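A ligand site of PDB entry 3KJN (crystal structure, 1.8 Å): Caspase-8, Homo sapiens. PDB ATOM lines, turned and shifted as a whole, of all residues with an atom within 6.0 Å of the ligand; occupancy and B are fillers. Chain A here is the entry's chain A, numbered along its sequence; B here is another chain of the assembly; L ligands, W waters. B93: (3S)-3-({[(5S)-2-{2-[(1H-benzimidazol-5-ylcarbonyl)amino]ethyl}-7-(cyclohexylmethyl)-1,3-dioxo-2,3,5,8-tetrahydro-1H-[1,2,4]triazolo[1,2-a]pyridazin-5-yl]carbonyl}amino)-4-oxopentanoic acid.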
ATOM      1  N   ARG A  48     -14.093  -6.242  19.909  1.00  0.00           N
ATOM      2  CA  ARG A  48     -14.691  -7.071  20.955  1.00  0.00           C
ATOM      3  C   ARG A  48     -14.540  -6.486  22.361  1.00  0.00           C
ATOM      4  O   ARG A  48     -13.591  -5.765  22.644  1.00  0.00           O
ATOM      5  CB  ARG A  48     -14.059  -8.464  20.915  1.00  0.00           C
ATOM      6  CG  ARG A  48     -14.481  -9.308  19.712  1.00  0.00           C
ATOM      7  CD  ARG A  48     -13.699 -10.608  19.647  1.00  0.00           C
ATOM      8  N   ARG A  50     -13.371  -6.673  26.104  1.00  0.00           N
ATOM      9  CA  ARG A  50     -12.085  -7.237  26.541  1.00  0.00           C
ATOM     10  C   ARG A  50     -12.251  -8.116  27.780  1.00  0.00           C
ATOM     11  O   ARG A  50     -11.737  -7.820  28.866  1.00  0.00           O
ATOM     12  CB  ARG A  50     -11.064  -6.122  26.763  1.00  0.00           C
ATOM     13  CG  ARG A  50     -10.718  -5.376  25.460  1.00  0.00           C
ATOM     14  CD  ARG A  50      -9.584  -4.360  25.622  1.00  0.00           C
ATOM     15  NE  ARG A  50      -8.346  -5.004  26.090  1.00  0.00           N
ATOM     16  CZ  ARG A  50      -7.937  -5.031  27.360  1.00  0.00           C
ATOM     17  NH1 ARG A  50      -8.571  -4.377  28.317  1.00  0.00           N
ATOM     18  NH2 ARG A  50      -6.837  -5.683  27.671  1.00  0.00           N
ATOM     19  N   SER A 106      -6.286  -1.814  27.199  1.00  0.00           N
ATOM     20  CA  SER A 106      -7.262  -1.506  26.164  1.00  0.00           C
ATOM     21  C   SER A 106      -6.932  -2.175  24.841  1.00  0.00           C
ATOM     22  O   SER A 106      -5.923  -2.867  24.706  1.00  0.00           O
ATOM     23  CB  SER A 106      -7.354   0.011  25.956  1.00  0.00           C
ATOM     24  OG  SER A 106      -8.546   0.394  25.296  1.00  0.00           O
ATOM     25  N   HIS A 107      -7.795  -1.956  23.853  1.00  0.00           N
ATOM     26  CA  HIS A 107      -7.443  -2.231  22.473  1.00  0.00           C
ATOM     27  C   HIS A 107      -6.501  -1.136  21.974  1.00  0.00           C
ATOM     28  O   HIS A 107      -6.437  -0.037  22.541  1.00  0.00           O
ATOM     29  CB  HIS A 107      -8.687  -2.279  21.585  1.00  0.00           C
ATOM     30  CG  HIS A 107      -9.530  -3.499  21.775  1.00  0.00           C
ATOM     31  ND1 HIS A 107      -9.051  -4.778  21.577  1.00  0.00           N
ATOM     32  CD2 HIS A 107     -10.829  -3.630  22.130  1.00  0.00           C
ATOM     33  CE1 HIS A 107     -10.023  -5.649  21.807  1.00  0.00           C
ATOM     34  NE2 HIS A 107     -11.113  -4.976  22.148  1.00  0.00           N
ATOM     35  N   GLY A 108      -5.785  -1.440  20.899  1.00  0.00           N
ATOM     36  CA  GLY A 108      -4.934  -0.458  20.246  1.00  0.00           C
ATOM     37  C   GLY A 108      -4.586  -0.815  18.816  1.00  0.00           C
ATOM     38  O   GLY A 108      -5.045  -1.819  18.270  1.00  0.00           O
ATOM     39  N   ASP A 109      -3.771   0.042  18.221  1.00  0.00           N
ATOM     40  CA  ASP A 109      -3.234  -0.142  16.882  1.00  0.00           C
ATOM     41  C   ASP A 109      -1.905   0.623  16.863  1.00  0.00           C
ATOM     42  O   ASP A 109      -1.470   1.106  17.900  1.00  0.00           O
ATOM     43  CB  ASP A 109      -4.210   0.408  15.833  1.00  0.00           C
ATOM     44  CG  ASP A 109      -4.046  -0.233  14.448  1.00  0.00           C
ATOM     45  OD1 ASP A 109      -2.918  -0.574  14.038  1.00  0.00           O
ATOM     46  OD2 ASP A 109      -5.065  -0.345  13.731  1.00  0.00           O
ATOM     47  N   GLN A 148      -0.855  -2.317  27.791  1.00  0.00           N
ATOM     48  CA  GLN A 148      -1.353  -3.586  27.321  1.00  0.00           C
ATOM     49  C   GLN A 148      -2.435  -3.322  26.271  1.00  0.00           C
ATOM     50  O   GLN A 148      -3.563  -2.935  26.594  1.00  0.00           O
ATOM     51  CB  GLN A 148      -1.897  -4.426  28.493  1.00  0.00           C
ATOM     52  CG  GLN A 148      -2.700  -5.666  28.092  1.00  0.00           C
ATOM     53  CD  GLN A 148      -1.992  -6.533  27.068  1.00  0.00           C
ATOM     54  OE1 GLN A 148      -0.816  -6.873  27.218  1.00  0.00           O
ATOM     55  NE2 GLN A 148      -2.705  -6.899  26.009  1.00  0.00           N
ATOM     56  N   ALA A 149      -2.036  -3.500  25.009  1.00  0.00           N
ATOM     57  CA  ALA A 149      -2.880  -3.302  23.848  1.00  0.00           C
ATOM     58  C   ALA A 149      -2.165  -3.907  22.641  1.00  0.00           C
ATOM     59  O   ALA A 149      -0.939  -4.075  22.671  1.00  0.00           O
ATOM     60  CB  ALA A 149      -3.123  -1.815  23.608  1.00  0.00           C
ATOM     61  N   CYS A 150      -2.911  -4.222  21.587  1.00  0.00           N
ATOM     62  CA  CYS A 150      -2.287  -4.503  20.286  1.00  0.00           C
ATOM     63  C   CYS A 150      -1.664  -3.199  19.755  1.00  0.00           C
ATOM     64  O   CYS A 150      -2.067  -2.100  20.140  1.00  0.00           O
ATOM     65  CB  CYS A 150      -3.297  -4.987  19.242  1.00  0.00           C
ATOM     66  SG  CYS A 150      -4.075  -6.606  19.512  1.00  0.00           S
ATOM     67  N   GLN A 151      -0.688  -3.349  18.872  1.00  0.00           N
ATOM     68  CA  GLN A 151      -0.125  -2.215  18.148  1.00  0.00           C
ATOM     69  C   GLN A 151      -0.214  -2.453  16.637  1.00  0.00           C
ATOM     70  O   GLN A 151       0.606  -1.953  15.872  1.00  0.00           O
ATOM     71  CB  GLN A 151       1.325  -1.976  18.588  1.00  0.00           C
ATOM     72  CG  GLN A 151       1.424  -1.434  19.999  1.00  0.00           C
ATOM     73  CD  GLN A 151       0.889  -0.020  20.105  1.00  0.00           C
ATOM     74  OE1 GLN A 151       1.531   0.932  19.655  1.00  0.00           O
ATOM     75  NE2 GLN A 151      -0.305   0.116  20.685  1.00  0.00           N
ATOM     76  N   GLY A 152      -1.254  -3.178  16.236  1.00  0.00           N
ATOM     77  CA  GLY A 152      -1.446  -3.572  14.846  1.00  0.00           C
ATOM     78  C   GLY A 152      -2.149  -4.912  14.785  1.00  0.00           C
ATOM     79  O   GLY A 152      -2.426  -5.511  15.827  1.00  0.00           O
ATOM     80  N   ASP A 153      -2.419  -5.379  13.573  1.00  0.00           N
ATOM     81  CA  ASP A 153      -3.201  -6.603  13.391  1.00  0.00           C
ATOM     82  C   ASP A 153      -2.392  -7.817  12.926  1.00  0.00           C
ATOM     83  O   ASP A 153      -2.964  -8.851  12.618  1.00  0.00           O
ATOM     84  CB  ASP A 153      -4.384  -6.344  12.433  1.00  0.00           C
ATOM     85  CG  ASP A 153      -3.960  -6.132  10.976  1.00  0.00           C
ATOM     86  OD1 ASP A 153      -2.756  -5.935  10.679  1.00  0.00           O
ATOM     87  OD2 ASP A 153      -4.858  -6.149  10.095  1.00  0.00           O
ATOM     88  N   TYR A 155       0.077 -11.049  13.226  1.00  0.00           N
ATOM     89  CA  TYR A 155       0.506 -12.099  14.137  1.00  0.00           C
ATOM     90  C   TYR A 155       2.022 -12.227  13.994  1.00  0.00           C
ATOM     91  O   TYR A 155       2.506 -12.616  12.946  1.00  0.00           O
ATOM     92  CB  TYR A 155      -0.151 -13.435  13.784  1.00  0.00           C
ATOM     93  CG  TYR A 155      -1.661 -13.438  13.936  1.00  0.00           C
ATOM     94  CD1 TYR A 155      -2.251 -13.268  15.172  1.00  0.00           C
ATOM     95  CD2 TYR A 155      -2.490 -13.620  12.824  1.00  0.00           C
ATOM     96  CE1 TYR A 155      -3.625 -13.251  15.320  1.00  0.00           C
ATOM     97  CE2 TYR A 155      -3.879 -13.616  12.957  1.00  0.00           C
ATOM     98  CZ  TYR A 155      -4.437 -13.421  14.213  1.00  0.00           C
ATOM     99  OH  TYR A 155      -5.811 -13.416  14.373  1.00  0.00           O
ATOM    100  N   VAL B  26      -0.015  -7.898  17.273  1.00  0.00           N
ATOM    101  CA  VAL B  26      -1.022  -8.159  18.274  1.00  0.00           C
ATOM    102  C   VAL B  26      -0.399  -8.561  19.623  1.00  0.00           C
ATOM    103  O   VAL B  26       0.733  -9.059  19.681  1.00  0.00           O
ATOM    104  CB  VAL B  26      -2.011  -9.280  17.809  1.00  0.00           C
ATOM    105  CG1 VAL B  26      -2.633  -8.913  16.463  1.00  0.00           C
ATOM    106  CG2 VAL B  26      -1.320 -10.629  17.713  1.00  0.00           C
ATOM    107  N   SER B  27      -1.129  -8.296  20.706  1.00  0.00           N
ATOM    108  CA  SER B  27      -0.844  -8.898  21.996  1.00  0.00           C
ATOM    109  C   SER B  27      -2.074  -9.661  22.445  1.00  0.00           C
ATOM    110  O   SER B  27      -3.192  -9.409  21.959  1.00  0.00           O
ATOM    111  CB  SER B  27      -0.471  -7.834  23.030  1.00  0.00           C
ATOM    112  OG  SER B  27      -1.576  -6.997  23.313  1.00  0.00           O
ATOM    113  N   TYR B  28      -1.873 -10.582  23.383  1.00  0.00           N
ATOM    114  CA  TYR B  28      -2.889 -11.571  23.731  1.00  0.00           C
ATOM    115  C   TYR B  28      -3.494 -11.426  25.122  1.00  0.00           C
ATOM    116  O   TYR B  28      -2.797 -11.073  26.080  1.00  0.00           O
ATOM    117  CB  TYR B  28      -2.309 -12.970  23.598  1.00  0.00           C
ATOM    118  CG  TYR B  28      -2.025 -13.372  22.168  1.00  0.00           C
ATOM    119  CD1 TYR B  28      -3.032 -13.901  21.363  1.00  0.00           C
ATOM    120  CD2 TYR B  28      -0.755 -13.234  21.621  1.00  0.00           C
ATOM    121  CE1 TYR B  28      -2.784 -14.288  20.047  1.00  0.00           C
ATOM    122  CE2 TYR B  28      -0.483 -13.609  20.293  1.00  0.00           C
ATOM    123  CZ  TYR B  28      -1.504 -14.135  19.525  1.00  0.00           C
ATOM    124  OH  TYR B  28      -1.264 -14.530  18.217  1.00  0.00           O
ATOM    125  N   ARG B  29      -4.784 -11.743  25.214  1.00  0.00           N
ATOM    126  CA  ARG B  29      -5.522 -11.749  26.470  1.00  0.00           C
ATOM    127  C   ARG B  29      -6.215 -13.099  26.615  1.00  0.00           C
ATOM    128  O   ARG B  29      -7.084 -13.428  25.817  1.00  0.00           O
ATOM    129  CB  ARG B  29      -6.564 -10.621  26.471  1.00  0.00           C
ATOM    130  CG  ARG B  29      -7.519 -10.585  27.688  1.00  0.00           C
ATOM    131  CD  ARG B  29      -8.371  -9.301  27.718  1.00  0.00           C
ATOM    132  NE  ARG B  29      -8.659  -8.881  26.352  1.00  0.00           N
ATOM    133  CZ  ARG B  29      -9.522  -9.475  25.549  1.00  0.00           C
ATOM    134  NH1 ARG B  29     -10.292 -10.480  25.967  1.00  0.00           N
ATOM    135  NH2 ARG B  29      -9.645  -9.046  24.307  1.00  0.00           N
ATOM    136  N   ASN B  30      -5.817 -13.871  27.616  1.00  0.00           N
ATOM    137  CA  ASN B  30      -6.537 -15.090  27.990  1.00  0.00           C
ATOM    138  C   ASN B  30      -7.726 -14.643  28.862  1.00  0.00           C
ATOM    139  O   ASN B  30      -7.512 -14.203  29.991  1.00  0.00           O
ATOM    140  CB  ASN B  30      -5.611 -16.043  28.756  1.00  0.00           C
ATOM    141  CG  ASN B  30      -6.273 -17.370  29.104  1.00  0.00           C
ATOM    142  OD1 ASN B  30      -5.602 -18.322  29.522  1.00  0.00           O
ATOM    143  ND2 ASN B  30      -7.585 -17.445  28.928  1.00  0.00           N
ATOM    144  N   PRO B  31      -8.965 -14.766  28.343  1.00  0.00           N
ATOM    145  CA  PRO B  31     -10.124 -14.311  29.120  1.00  0.00           C
ATOM    146  C   PRO B  31     -10.251 -14.935  30.517  1.00  0.00           C
ATOM    147  O   PRO B  31     -10.874 -14.334  31.395  1.00  0.00           O
ATOM    148  CB  PRO B  31     -11.314 -14.720  28.241  1.00  0.00           C
ATOM    149  CG  PRO B  31     -10.765 -14.780  26.867  1.00  0.00           C
ATOM    150  CD  PRO B  31      -9.370 -15.320  27.034  1.00  0.00           C
ATOM    151  N   THR B  35      -3.872 -11.010  30.588  1.00  0.00           N
ATOM    152  CA  THR B  35      -2.990 -10.901  29.432  1.00  0.00           C
ATOM    153  C   THR B  35      -1.633 -11.556  29.678  1.00  0.00           C
ATOM    154  O   THR B  35      -1.143 -11.584  30.807  1.00  0.00           O
ATOM    155  CB  THR B  35      -2.809  -9.437  28.955  1.00  0.00           C
ATOM    156  OG1 THR B  35      -2.241  -8.638  30.000  1.00  0.00           O
ATOM    157  CG2 THR B  35      -4.154  -8.830  28.514  1.00  0.00           C
ATOM    158  N   TRP B  36      -1.040 -12.082  28.614  1.00  0.00           N
ATOM    159  CA  TRP B  36       0.303 -12.640  28.699  1.00  0.00           C
ATOM    160  C   TRP B  36       1.253 -11.622  29.327  1.00  0.00           C
ATOM    161  O   TRP B  36       2.002 -11.954  30.249  1.00  0.00           O
ATOM    162  CB  TRP B  36       0.845 -13.037  27.310  1.00  0.00           C
ATOM    163  CG  TRP B  36       0.170 -14.199  26.673  1.00  0.00           C
ATOM    164  CD1 TRP B  36      -0.826 -14.972  27.198  1.00  0.00           C
ATOM    165  CD2 TRP B  36       0.476 -14.758  25.389  1.00  0.00           C
ATOM    166  NE1 TRP B  36      -1.177 -15.965  26.307  1.00  0.00           N
ATOM    167  CE2 TRP B  36      -0.392 -15.867  25.191  1.00  0.00           C
ATOM    168  CE3 TRP B  36       1.399 -14.440  24.375  1.00  0.00           C
ATOM    169  CZ2 TRP B  36      -0.368 -16.635  24.029  1.00  0.00           C
ATOM    170  CZ3 TRP B  36       1.415 -15.216  23.221  1.00  0.00           C
ATOM    171  CH2 TRP B  36       0.532 -16.286  23.058  1.00  0.00           C
ATOM    172  N   ASP B  70       2.797 -19.277  23.057  1.00  0.00           N
ATOM    173  CA  ASP B  70       2.342 -19.257  21.674  1.00  0.00           C
ATOM    174  C   ASP B  70       0.841 -19.370  21.517  1.00  0.00           C
ATOM    175  O   ASP B  70       0.122 -19.839  22.412  1.00  0.00           O
ATOM    176  CB  ASP B  70       3.065 -20.305  20.837  1.00  0.00           C
ATOM    177  CG  ASP B  70       3.083 -21.648  21.487  1.00  0.00           C
ATOM    178  OD1 ASP B  70       1.993 -22.125  21.885  1.00  0.00           O
ATOM    179  OD2 ASP B  70       4.173 -22.235  21.610  1.00  0.00           O
HETATM  180  C1  B93 L   1      -5.861  -6.319  19.462  1.00  0.00           C
HETATM  181  C2  B93 L   1      -5.953  -5.798  20.858  1.00  0.00           C
HETATM  182  O3  B93 L   1      -5.796  -4.597  21.069  1.00  0.00           O
HETATM  183  C4  B93 L   1      -6.257  -6.760  21.987  1.00  0.00           C
HETATM  184  C5  B93 L   1      -5.461  -6.347  23.213  1.00  0.00           C
HETATM  185  C6  B93 L   1      -6.167  -6.899  24.416  1.00  0.00           C
HETATM  186  O7  B93 L   1      -7.349  -7.201  24.471  1.00  0.00           O
HETATM  187  O8  B93 L   1      -5.335  -7.019  25.472  1.00  0.00           O
HETATM  188  N9  B93 L   1      -5.821  -8.073  21.540  1.00  0.00           N
HETATM  189  C10 B93 L   1      -6.740  -9.052  21.262  1.00  0.00           C
HETATM  190  O11 B93 L   1      -7.950  -8.950  21.401  1.00  0.00           O
HETATM  191  C12 B93 L   1      -6.068 -10.300  20.749  1.00  0.00           C
HETATM  192  C13 B93 L   1      -5.836 -10.132  19.278  1.00  0.00           C
HETATM  193  C14 B93 L   1      -6.559 -10.735  18.325  1.00  0.00           C
HETATM  194  C15 B93 L   1      -6.223 -10.513  16.889  1.00  0.00           C
HETATM  195  C16 B93 L   1      -7.219  -9.762  16.034  1.00  0.00           C
HETATM  196  C17 B93 L   1      -7.664  -8.455  16.648  1.00  0.00           C
HETATM  197  C18 B93 L   1      -8.668  -7.773  15.741  1.00  0.00           C
HETATM  198  C19 B93 L   1      -8.053  -7.504  14.382  1.00  0.00           C
HETATM  199  C20 B93 L   1      -7.568  -8.797  13.750  1.00  0.00           C
HETATM  200  C21 B93 L   1      -6.585  -9.504  14.672  1.00  0.00           C
HETATM  201  C22 B93 L   1      -7.689 -11.652  18.670  1.00  0.00           C
HETATM  202  N23 B93 L   1      -8.051 -11.488  20.063  1.00  0.00           N
HETATM  203  N24 B93 L   1      -6.974 -11.418  20.942  1.00  0.00           N
HETATM  204  C25 B93 L   1      -7.386 -11.868  22.172  1.00  0.00           C
HETATM  205  O26 B93 L   1      -6.821 -11.723  23.244  1.00  0.00           O
HETATM  206  N27 B93 L   1      -8.618 -12.438  21.959  1.00  0.00           N
HETATM  207  C28 B93 L   1      -9.510 -12.782  23.040  1.00  0.00           C
HETATM  208  C29 B93 L   1      -9.581 -14.277  23.229  1.00  0.00           C
HETATM  209  N30 B93 L   1      -8.316 -14.830  23.669  1.00  0.00           N
HETATM  210  C31 B93 L   1      -8.136 -16.201  23.719  1.00  0.00           C
HETATM  211  O32 B93 L   1      -8.925 -17.035  23.299  1.00  0.00           O
HETATM  212  C33 B93 L   1      -6.874 -16.629  24.353  1.00  0.00           C
HETATM  213  C34 B93 L   1      -5.766 -15.815  24.252  1.00  0.00           C
HETATM  214  C35 B93 L   1      -4.556 -16.140  24.829  1.00  0.00           C
HETATM  215  C36 B93 L   1      -4.548 -17.333  25.510  1.00  0.00           C
HETATM  216  N37 B93 L   1      -3.549 -17.970  26.188  1.00  0.00           N
HETATM  217  C38 B93 L   1      -4.053 -19.139  26.680  1.00  0.00           C
HETATM  218  N39 B93 L   1      -5.321 -19.285  26.354  1.00  0.00           N
HETATM  219  C40 B93 L   1      -5.645 -18.166  25.616  1.00  0.00           C
HETATM  220  C41 B93 L   1      -6.858 -17.827  25.037  1.00  0.00           C
HETATM  221  C42 B93 L   1      -9.040 -12.241  20.663  1.00  0.00           C
HETATM  222  O43 B93 L   1     -10.075 -12.658  20.150  1.00  0.00           O
HETATM  223  O   HOH W   1      -6.925 -21.422  26.790  1.00  0.00           O
HETATM  224  O   HOH W   2     -11.037 -10.833  17.657  1.00  0.00           O
HETATM  225  O   HOH W   3     -11.816 -17.258  23.697  1.00  0.00           O
HETATM  226  O   HOH W   4      -9.044  -5.237  18.547  1.00  0.00           O
HETATM  227  O   HOH W   5     -10.410  -9.203  19.997  1.00  0.00           O
HETATM  228  O   HOH W   6     -11.440 -10.198  22.280  1.00  0.00           O
HETATM  229  O   HOH W   7     -12.392 -12.336  24.862  1.00  0.00           O
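Ser 106 touches the ligand (O to C5, 3.8 Å).
Tyr 155 touches the ligand (OH to C15, 3.9 Å).
Val 26 of chain B touches the ligand.
C of Tyr 28 of chain B touches O26 of the ligand, at 3.8 Å.
CD of Pro 31 of chain B touches N30 of the ligand, 3.6 Å away.
Thr 35 of chain B touches the ligand (CG2 to O8, 3.7 Å).
Hydrophobic or aromatic side chains within 4 Å of the ligand: His 107, Val 26 of chain B, Pro 31 of chain B and Trp 36 of chain B.
Within 4 Å of the ligand: Arg 50, Ser 106, His 107, Gly 108, Gln 148, Cys 150, Tyr 155, Val 26 of chain B, Ser 27 of chain B, Tyr 28 of chain B, Arg 29 of chain B, Asn 30 of chain B, Pro 31 of chain B, Thr 35 of chain B and Trp 36 of chain B.
Along chain A the residues within 4 Å of the ligand span positions 50 to 155.
The nearest printed residue that does not touch the ligand is Ala 149 (4.02 Å).
The backbone carbonyl oxygen of Gln 148 lies within hydrogen-bond range of the backbone NH of Ser 106, 3.0 Å away.
The side-chain hydroxyl (OG) of Ser 27 of chain B lies within hydrogen-bond range of the backbone carbonyl oxygen (O) of Ala 149 (3.1 Å).
The side-chain hydroxyl (OG) of Ser 27 of chain B lies within hydrogen-bond range of the side-chain amide nitrogen (NE2) of Gln 148, at 2.9 Å.
The side-chain sulfur (SG) of Cys 150 is in hydrogen-bond range of the backbone NH (N) of Ser 27 of chain B.
N of Trp 36 of chain B sits at hydrogen-bond distance from O of Tyr 28 of chain B (3.2 Å).
The backbone NH (N) of Asp 109 sits at hydrogen-bond distance from the backbone carbonyl oxygen (O) of Cys 150 (3.3 Å).
A ring nitrogen (NE2) of His 107 sits at hydrogen-bond distance from the backbone carbonyl oxygen (O) of Arg 48, at 2.6 Å.
The backbone NH of Cys 150 is in hydrogen-bond range of an oxygen (O3) of the ligand, 3.0 Å away.
An oxygen (O8) of the ligand is in hydrogen-bond range of the side-chain amide nitrogen (NE2) of Gln 148.
SG of Cys 150 is covalently linked to C1 of the ligand (1.8 Å).
The guanidinium group of Arg 29 of chain B lies within salt-bridge range of an oxygen (O7) of the ligand (2.8 Å).
The side-chain amide oxygen (OD1) of Asn 30 of chain B lies close to a nitrogen (N39) of the ligand (3.3 Å).
The backbone carbonyl oxygen (O) of Ser 27 of chain B sits at hydrogen-bond distance from a nitrogen (N9) of the ligand, 3.0 Å away.
The guanidinium group (NE) of Arg 50 lies within salt-bridge range of an oxygen (O7) of the ligand.
N of Gly 108 sits at hydrogen-bond distance from O3 of the ligand (3.2 Å).
ND1 of His 107 lies close to O3 of the ligand (3.3 Å).
The backbone NH (N) of Arg 29 of chain B lies within hydrogen-bond range of an oxygen (O26) of the ligand.
The indole nitrogen (NE1) of Trp 36 of chain B lies close to a nitrogen (N37) of the ligand (3.1 Å).
O of Arg 29 of chain B is in hydrogen-bond range of N30 of the ligand (2.8 Å).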
